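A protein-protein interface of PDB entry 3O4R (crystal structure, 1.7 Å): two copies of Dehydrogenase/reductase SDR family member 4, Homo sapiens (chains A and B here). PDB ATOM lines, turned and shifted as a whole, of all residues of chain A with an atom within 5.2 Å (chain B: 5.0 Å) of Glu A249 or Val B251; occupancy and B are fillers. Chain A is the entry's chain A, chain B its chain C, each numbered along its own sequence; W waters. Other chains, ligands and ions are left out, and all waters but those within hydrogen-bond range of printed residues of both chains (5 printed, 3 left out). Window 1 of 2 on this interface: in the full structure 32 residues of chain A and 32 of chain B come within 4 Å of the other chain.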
ATOM      1  N   THR A 176     -14.477   0.154  10.936  1.00  0.00           N
ATOM      2  CA  THR A 176     -13.324   0.754  11.604  1.00  0.00           C
ATOM      3  C   THR A 176     -11.980   0.164  11.119  1.00  0.00           C
ATOM      4  O   THR A 176     -11.048   0.898  10.760  1.00  0.00           O
ATOM      5  CB  THR A 176     -13.460   0.596  13.135  1.00  0.00           C
ATOM      6  OG1 THR A 176     -14.673   1.198  13.596  1.00  0.00           O
ATOM      7  CG2 THR A 176     -12.323   1.269  13.850  1.00  0.00           C
ATOM      8  N   LYS A 177     -11.904  -1.164  11.093  1.00  0.00           N
ATOM      9  CA  LYS A 177     -10.714  -1.904  10.654  1.00  0.00           C
ATOM     10  C   LYS A 177     -10.413  -1.584   9.184  1.00  0.00           C
ATOM     11  O   LYS A 177      -9.296  -1.255   8.817  1.00  0.00           O
ATOM     12  CB  LYS A 177     -10.904  -3.438  10.845  1.00  0.00           C
ATOM     13  CG  LYS A 177     -10.854  -3.956  12.280  1.00  0.00           C
ATOM     14  CD  LYS A 177      -9.471  -3.743  12.944  1.00  0.00           C
ATOM     15  CE  LYS A 177      -9.353  -4.504  14.269  1.00  0.00           C
ATOM     16  NZ  LYS A 177      -8.101  -4.146  15.054  1.00  0.00           N
ATOM     17  N   VAL A 190      -8.083   5.835  12.331  1.00  0.00           N
ATOM     18  CA  VAL A 190      -9.512   5.485  12.467  1.00  0.00           C
ATOM     19  C   VAL A 190      -9.673   4.447  13.591  1.00  0.00           C
ATOM     20  O   VAL A 190      -9.144   3.324  13.510  1.00  0.00           O
ATOM     21  CB  VAL A 190     -10.096   4.925  11.177  1.00  0.00           C
ATOM     22  CG1 VAL A 190     -11.581   4.774  11.340  1.00  0.00           C
ATOM     23  CG2 VAL A 190      -9.762   5.853   9.978  1.00  0.00           C
ATOM     24  N   ASN A 191     -10.363   4.861  14.639  1.00  0.00           N
ATOM     25  CA  ASN A 191     -10.580   4.065  15.854  1.00  0.00           C
ATOM     26  C   ASN A 191     -12.067   4.022  16.219  1.00  0.00           C
ATOM     27  O   ASN A 191     -12.888   4.727  15.624  1.00  0.00           O
ATOM     28  CB  ASN A 191      -9.723   4.612  16.984  1.00  0.00           C
ATOM     29  CG  ASN A 191      -8.252   4.408  16.722  1.00  0.00           C
ATOM     30  OD1 ASN A 191      -7.795   3.273  16.572  1.00  0.00           O
ATOM     31  ND2 ASN A 191      -7.489   5.506  16.664  1.00  0.00           N
ATOM     32  N   CYS A 192     -12.399   3.215  17.217  1.00  0.00           N
ATOM     33  CA  CYS A 192     -13.763   2.984  17.590  1.00  0.00           C
ATOM     34  C   CYS A 192     -13.950   3.000  19.121  1.00  0.00           C
ATOM     35  O   CYS A 192     -13.123   2.478  19.879  1.00  0.00           O
ATOM     36  CB  CYS A 192     -14.204   1.659  16.992  1.00  0.00           C
ATOM     37  SG  CYS A 192     -15.845   1.105  17.488  1.00  0.00           S
ATOM     38  N   ILE A 246      -1.817   4.598  17.427  1.00  0.00           N
ATOM     39  CA  ILE A 246      -3.033   3.827  17.617  1.00  0.00           C
ATOM     40  C   ILE A 246      -3.990   4.108  16.464  1.00  0.00           C
ATOM     41  O   ILE A 246      -4.520   5.218  16.315  1.00  0.00           O
ATOM     42  CB  ILE A 246      -3.711   4.142  18.960  1.00  0.00           C
ATOM     43  CG1 ILE A 246      -2.710   4.010  20.108  1.00  0.00           C
ATOM     44  CG2 ILE A 246      -4.912   3.183  19.171  1.00  0.00           C
ATOM     45  CD1 ILE A 246      -3.201   4.470  21.428  1.00  0.00           C
ATOM     46  N   THR A 247      -4.212   3.083  15.650  1.00  0.00           N
ATOM     47  CA  THR A 247      -5.178   3.169  14.582  1.00  0.00           C
ATOM     48  C   THR A 247      -5.701   1.770  14.407  1.00  0.00           C
ATOM     49  O   THR A 247      -5.016   0.829  14.769  1.00  0.00           O
ATOM     50  CB  THR A 247      -4.586   3.691  13.262  1.00  0.00           C
ATOM     51  OG1 THR A 247      -5.658   4.063  12.404  1.00  0.00           O
ATOM     52  CG2 THR A 247      -3.691   2.660  12.564  1.00  0.00           C
ATOM     53  N   GLY A 248      -6.916   1.651  13.894  1.00  0.00           N
ATOM     54  CA  GLY A 248      -7.570   0.363  13.775  1.00  0.00           C
ATOM     55  C   GLY A 248      -8.009  -0.278  15.092  1.00  0.00           C
ATOM     56  O   GLY A 248      -8.312  -1.470  15.125  1.00  0.00           O
ATOM     57  N   GLU A 249      -8.116   0.512  16.154  1.00  0.00           N
ATOM     58  CA  GLU A 249      -8.371  -0.007  17.499  1.00  0.00           C
ATOM     59  C   GLU A 249      -9.771   0.341  18.036  1.00  0.00           C
ATOM     60  O   GLU A 249     -10.186   1.516  18.001  1.00  0.00           O
ATOM     61  CB  GLU A 249      -7.316   0.576  18.437  1.00  0.00           C
ATOM     62  CG  GLU A 249      -7.288  -0.015  19.828  1.00  0.00           C
ATOM     63  CD  GLU A 249      -6.839  -1.465  19.846  1.00  0.00           C
ATOM     64  OE1 GLU A 249      -6.443  -1.982  18.761  1.00  0.00           O
ATOM     65  OE2 GLU A 249      -6.889  -2.070  20.952  1.00  0.00           O
ATOM     66  N   THR A 250     -10.495  -0.676  18.522  1.00  0.00           N
ATOM     67  CA  THR A 250     -11.714  -0.470  19.287  1.00  0.00           C
ATOM     68  C   THR A 250     -11.399  -0.525  20.794  1.00  0.00           C
ATOM     69  O   THR A 250     -10.749  -1.473  21.279  1.00  0.00           O
ATOM     70  CB  THR A 250     -12.798  -1.532  18.933  1.00  0.00           C
ATOM     71  OG1 THR A 250     -13.127  -1.424  17.545  1.00  0.00           O
ATOM     72  CG2 THR A 250     -14.091  -1.330  19.770  1.00  0.00           C
ATOM     73  N   VAL A 251     -11.800   0.519  21.516  1.00  0.00           N
ATOM     74  CA  VAL A 251     -11.662   0.570  22.959  1.00  0.00           C
ATOM     75  C   VAL A 251     -13.038   0.477  23.594  1.00  0.00           C
ATOM     76  O   VAL A 251     -13.891   1.344  23.381  1.00  0.00           O
ATOM     77  CB  VAL A 251     -10.974   1.868  23.403  1.00  0.00           C
ATOM     78  CG1 VAL A 251     -10.684   1.839  24.902  1.00  0.00           C
ATOM     79  CG2 VAL A 251      -9.706   2.065  22.623  1.00  0.00           C
ATOM     80  N   ARG A 260     -14.384  -8.951  24.842  1.00  0.00           N
ATOM     81  CA  ARG A 260     -13.572  -9.876  24.096  1.00  0.00           C
ATOM     82  C   ARG A 260     -12.144  -9.700  24.564  1.00  0.00           C
ATOM     83  O   ARG A 260     -11.822  -8.707  25.225  1.00  0.00           O
ATOM     84  CB  ARG A 260     -13.681  -9.626  22.585  1.00  0.00           C
ATOM     85  CG  ARG A 260     -12.678  -8.644  21.980  1.00  0.00           C
ATOM     86  CD  ARG A 260     -12.812  -7.193  22.445  1.00  0.00           C
ATOM     87  NE  ARG A 260     -12.213  -6.307  21.445  1.00  0.00           N
ATOM     88  CZ  ARG A 260     -11.688  -5.094  21.672  1.00  0.00           C
ATOM     89  NH1 ARG A 260     -11.185  -4.396  20.665  1.00  0.00           N
ATOM     90  NH2 ARG A 260     -11.651  -4.562  22.875  1.00  0.00           N
ATOM     91  N   CYS B 192      -4.559  -3.831  30.138  1.00  0.00           N
ATOM     92  CA  CYS B 192      -3.376  -4.361  29.486  1.00  0.00           C
ATOM     93  C   CYS B 192      -2.991  -3.505  28.273  1.00  0.00           C
ATOM     94  O   CYS B 192      -3.844  -3.062  27.515  1.00  0.00           O
ATOM     95  CB  CYS B 192      -3.640  -5.811  29.091  1.00  0.00           C
ATOM     96  SG  CYS B 192      -2.443  -6.655  28.025  1.00  0.00           S
ATOM     97  N   LEU B 193      -1.696  -3.212  28.158  1.00  0.00           N
ATOM     98  CA  LEU B 193      -1.107  -2.611  26.966  1.00  0.00           C
ATOM     99  C   LEU B 193      -0.473  -3.686  26.109  1.00  0.00           C
ATOM    100  O   LEU B 193       0.375  -4.435  26.600  1.00  0.00           O
ATOM    101  CB  LEU B 193      -0.026  -1.605  27.397  1.00  0.00           C
ATOM    102  CG  LEU B 193       0.903  -1.044  26.327  1.00  0.00           C
ATOM    103  CD1 LEU B 193       0.195  -0.049  25.408  1.00  0.00           C
ATOM    104  CD2 LEU B 193       2.108  -0.388  27.018  1.00  0.00           C
ATOM    105  N   ALA B 194      -0.847  -3.737  24.826  1.00  0.00           N
ATOM    106  CA  ALA B 194      -0.314  -4.686  23.856  1.00  0.00           C
ATOM    107  C   ALA B 194       0.409  -3.928  22.732  1.00  0.00           C
ATOM    108  O   ALA B 194      -0.180  -3.567  21.713  1.00  0.00           O
ATOM    109  CB  ALA B 194      -1.430  -5.565  23.282  1.00  0.00           C
ATOM    110  N   ILE B 234      -1.371   6.201  26.728  1.00  0.00           N
ATOM    111  CA  ILE B 234      -2.501   5.338  26.992  1.00  0.00           C
ATOM    112  C   ILE B 234      -2.369   4.741  28.407  1.00  0.00           C
ATOM    113  O   ILE B 234      -3.355   4.669  29.150  1.00  0.00           O
ATOM    114  CB  ILE B 234      -2.653   4.281  25.891  1.00  0.00           C
ATOM    115  CG1 ILE B 234      -3.899   3.419  26.120  1.00  0.00           C
ATOM    116  CG2 ILE B 234      -1.417   3.382  25.814  1.00  0.00           C
ATOM    117  CD1 ILE B 234      -5.219   4.170  26.083  1.00  0.00           C
ATOM    118  N   LEU B 238      -5.042   5.151  31.415  1.00  0.00           N
ATOM    119  CA  LEU B 238      -5.661   3.999  32.061  1.00  0.00           C
ATOM    120  C   LEU B 238      -5.415   3.979  33.572  1.00  0.00           C
ATOM    121  O   LEU B 238      -6.255   3.504  34.327  1.00  0.00           O
ATOM    122  CB  LEU B 238      -5.150   2.697  31.455  1.00  0.00           C
ATOM    123  CG  LEU B 238      -5.539   2.443  30.008  1.00  0.00           C
ATOM    124  CD1 LEU B 238      -4.784   1.251  29.444  1.00  0.00           C
ATOM    125  CD2 LEU B 238      -7.070   2.243  29.938  1.00  0.00           C
ATOM    126  N   GLU B 249      -9.640  -4.444  29.985  1.00  0.00           N
ATOM    127  CA  GLU B 249      -9.463  -4.034  28.590  1.00  0.00           C
ATOM    128  C   GLU B 249      -8.007  -4.139  28.170  1.00  0.00           C
ATOM    129  O   GLU B 249      -7.140  -3.658  28.891  1.00  0.00           O
ATOM    130  CB  GLU B 249      -9.916  -2.573  28.446  1.00  0.00           C
ATOM    131  CG  GLU B 249      -9.958  -2.042  27.014  1.00  0.00           C
ATOM    132  CD  GLU B 249     -11.029  -2.708  26.169  1.00  0.00           C
ATOM    133  OE1 GLU B 249     -11.831  -3.493  26.754  1.00  0.00           O
ATOM    134  OE2 GLU B 249     -11.065  -2.432  24.935  1.00  0.00           O
ATOM    135  N   THR B 250      -7.756  -4.745  27.007  1.00  0.00           N
ATOM    136  CA  THR B 250      -6.442  -4.686  26.357  1.00  0.00           C
ATOM    137  C   THR B 250      -6.432  -3.657  25.230  1.00  0.00           C
ATOM    138  O   THR B 250      -7.236  -3.736  24.306  1.00  0.00           O
ATOM    139  CB  THR B 250      -6.049  -6.063  25.808  1.00  0.00           C
ATOM    140  OG1 THR B 250      -5.873  -6.970  26.897  1.00  0.00           O
ATOM    141  CG2 THR B 250      -4.763  -6.011  24.963  1.00  0.00           C
ATOM    142  N   VAL B 251      -5.514  -2.688  25.299  1.00  0.00           N
ATOM    143  CA  VAL B 251      -5.360  -1.701  24.240  1.00  0.00           C
ATOM    144  C   VAL B 251      -4.105  -1.965  23.404  1.00  0.00           C
ATOM    145  O   VAL B 251      -2.978  -1.986  23.921  1.00  0.00           O
ATOM    146  CB  VAL B 251      -5.270  -0.263  24.782  1.00  0.00           C
ATOM    147  CG1 VAL B 251      -5.207   0.711  23.618  1.00  0.00           C
ATOM    148  CG2 VAL B 251      -6.449   0.068  25.699  1.00  0.00           C
ATOM    149  N   VAL B 252      -4.298  -2.156  22.108  1.00  0.00           N
ATOM    150  CA  VAL B 252      -3.182  -2.419  21.199  1.00  0.00           C
ATOM    151  C   VAL B 252      -2.615  -1.105  20.684  1.00  0.00           C
ATOM    152  O   VAL B 252      -3.348  -0.257  20.198  1.00  0.00           O
ATOM    153  CB  VAL B 252      -3.617  -3.313  20.012  1.00  0.00           C
ATOM    154  CG1 VAL B 252      -2.503  -3.367  18.915  1.00  0.00           C
ATOM    155  CG2 VAL B 252      -3.986  -4.721  20.511  1.00  0.00           C
ATOM    156  N   VAL B 253      -1.303  -0.937  20.815  1.00  0.00           N
ATOM    157  CA  VAL B 253      -0.597   0.217  20.289  1.00  0.00           C
ATOM    158  C   VAL B 253       0.406  -0.302  19.256  1.00  0.00           C
ATOM    159  O   VAL B 253       1.595  -0.497  19.547  1.00  0.00           O
ATOM    160  CB  VAL B 253       0.118   0.976  21.405  1.00  0.00           C
ATOM    161  CG1 VAL B 253       0.900   2.177  20.836  1.00  0.00           C
ATOM    162  CG2 VAL B 253      -0.896   1.434  22.466  1.00  0.00           C
ATOM    163  N   SER B 259      -4.461  -7.112  14.588  1.00  0.00           N
ATOM    164  CA  SER B 259      -4.537  -7.710  15.920  1.00  0.00           C
ATOM    165  C   SER B 259      -5.840  -8.457  16.054  1.00  0.00           C
ATOM    166  O   SER B 259      -5.866  -9.673  15.854  1.00  0.00           O
ATOM    167  CB  SER B 259      -4.399  -6.646  17.009  1.00  0.00           C
ATOM    168  OG  SER B 259      -5.391  -5.656  16.888  1.00  0.00           O
ATOM    169  N   ARG B 260      -6.915  -7.741  16.370  1.00  0.00           N
ATOM    170  CA  ARG B 260      -8.243  -8.377  16.490  1.00  0.00           C
ATOM    171  C   ARG B 260      -9.407  -7.369  16.513  1.00  0.00           C
ATOM    172  O   ARG B 260      -9.210  -6.189  16.746  1.00  0.00           O
ATOM    173  CB  ARG B 260      -8.275  -9.265  17.738  1.00  0.00           C
ATOM    174  CG  ARG B 260      -8.738  -8.604  19.031  1.00  0.00           C
ATOM    175  CD  ARG B 260      -7.902  -7.443  19.530  1.00  0.00           C
ATOM    176  NE  ARG B 260      -8.266  -7.153  20.915  1.00  0.00           N
ATOM    177  CZ  ARG B 260      -8.028  -6.016  21.571  1.00  0.00           C
ATOM    178  NH1 ARG B 260      -7.414  -4.990  20.993  1.00  0.00           N
ATOM    179  NH2 ARG B 260      -8.399  -5.911  22.839  1.00  0.00           N
HETATM  180  O   HOH W   1      -5.091  -3.856  14.964  1.00  0.00           O
HETATM  181  O   HOH W   2      -9.739  -6.297  25.876  1.00  0.00           O
HETATM  182  O   HOH W   3      -3.130   0.159  17.552  1.00  0.00           O
HETATM  183  O   HOH W   4      -6.628  -6.150  13.180  1.00  0.00           O
HETATM  184  O   HOH W   5      -7.064  -4.308  18.446  1.00  0.00           O
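Printed residues of chain B that touch a printed residue of chain A: Glu B249, Thr B250, Val B251, Val B252, Val B253, Ser B259 and Arg B260. Hydrophobic or aromatic side chains of chain B that line the printed part of chain A: Val B252 and Val B253. Of the 12 printed residues of chain A, 6 touch a printed residue of chain B. Printed residues of chain A that touch a printed residue of chain B: Lys A177, Ile A246, Glu A249, Thr A250, Val A251 and Arg A260. Hydrophobic or aromatic side chains of chain A that line the printed part of chain B: Ile A246. Among the printed residues, 12 pairs touch across the chains. Among the printed residues, Asp or Glu carboxylates within 4 Å of a Lys or Arg side-chain nitrogen of the other chain: Glu A249 with Arg B260 and Arg A260 with Glu B249.
The side-chain amino group of Lys A177 sits at hydrogen-bond distance from the backbone carbonyl oxygen of Arg B260, 2.9 Å away. The side-chain carboxylate of Glu A249 sits at hydrogen-bond distance from the backbone NH of Val B252. The guanidinium group of Arg B260 is in salt-bridge range of the side-chain carboxylate of Glu A249 (3.0 Å). OE2 of Glu B249 is in salt-bridge range of NH2 of Arg A260, 3.0 Å away.
Glu A249 touches Thr B250, and with the chains exchanged Thr A250 touches Glu B249. Glu A249 touches Val B251, and with the chains exchanged Val A251 touches Glu B249. Glu A249 touches Arg B260, and with the chains exchanged Arg A260 touches Glu B249. Arg B260 touches its own counterpart, Arg A260. Of the 12 pairs that touch across the chains among the printed residues, 7 have their exchanged pair printed and touching as well.
NZ of Lys A177 sits at hydrogen-bond distance from O of Gly A248, at 2.7 Å. N of Cys A192 lies within hydrogen-bond range of O of Glu A249. O of Cys A192 sits at hydrogen-bond distance from N of Val A251 (2.9 Å). N of Cys B192 lies within hydrogen-bond range of O of Glu B249 (2.9 Å). N of Val B251 is in hydrogen-bond range of O of Cys B192. The backbone carbonyl oxygen (O) of Val B251 sits at hydrogen-bond distance from the backbone NH (N) of Ala B194, at 2.9 Å.
Among the printed residues, merely in contact across the chains: Arg A260 with Arg B260 (3.5 Å), Lys A177 with Ser B259 (3.6 Å), Val A251 with Glu B249 (3.6 Å), Glu A249 with Val B251 (3.6 Å), Glu A249 with Thr B250 (3.8 Å), Thr A250 with Glu B249 (3.8 Å), Ile A246 with Val B252 (3.9 Å) and Ile A246 with Val B253 (3.9 Å).
Thr A176 touches none of the printed residues of chain B. Printed residues of chain B within 4 Å of Lys A177: Ser B259 (3.6 Å) and Arg B260 (2.9 Å). Glu A249 touches just these residues of chain B: Thr B250 (3.8 Å), Val B251 (3.6 Å), Val B252 (2.8 Å) and Arg B260 (3.0 Å). Printed residues of chain B within 4 Å of Arg A260: Glu B249 (3.0 Å) and Arg B260 (3.5 Å). Leu B238 touches none of the printed residues of chain A. Printed residues of chain A within 4 Å of Val B253: Ile A246. The nearest residue of chain B that does not touch Glu A249 is Ser B259 (4.3 Å). The nearest printed residue of chain A that does not touch Arg B260 is Thr A250 (4.9 Å).
Water W5 lies within hydrogen-bond range of the side-chain carboxylate (OE1) of Glu A249 (2.4 Å), the side-chain hydroxyl (OG) of Ser B259 (2.7 Å) and the guanidinium group (NH1) of Arg B260 (2.7 Å). Water W1 bridges the side-chain hydroxyl (OG) of Ser B259 (2.7 Å) and the side-chain amino group (NZ) of Lys A177 (3.0 Å). Water W3 lies within hydrogen-bond range of O of Val B252 (2.7 Å) and O of Thr A247 (3.4 Å). Water W4 bridges the backbone NH (N) of Ser B259 (2.8 Å) and the side-chain amino group (NZ) of Lys A177 (3.1 Å). Water W2 lies within hydrogen-bond range of N of Thr B250 (2.8 Å), O of Arg A260 (3.3 Å) and NH2 of Arg B260 (3.3 Å).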
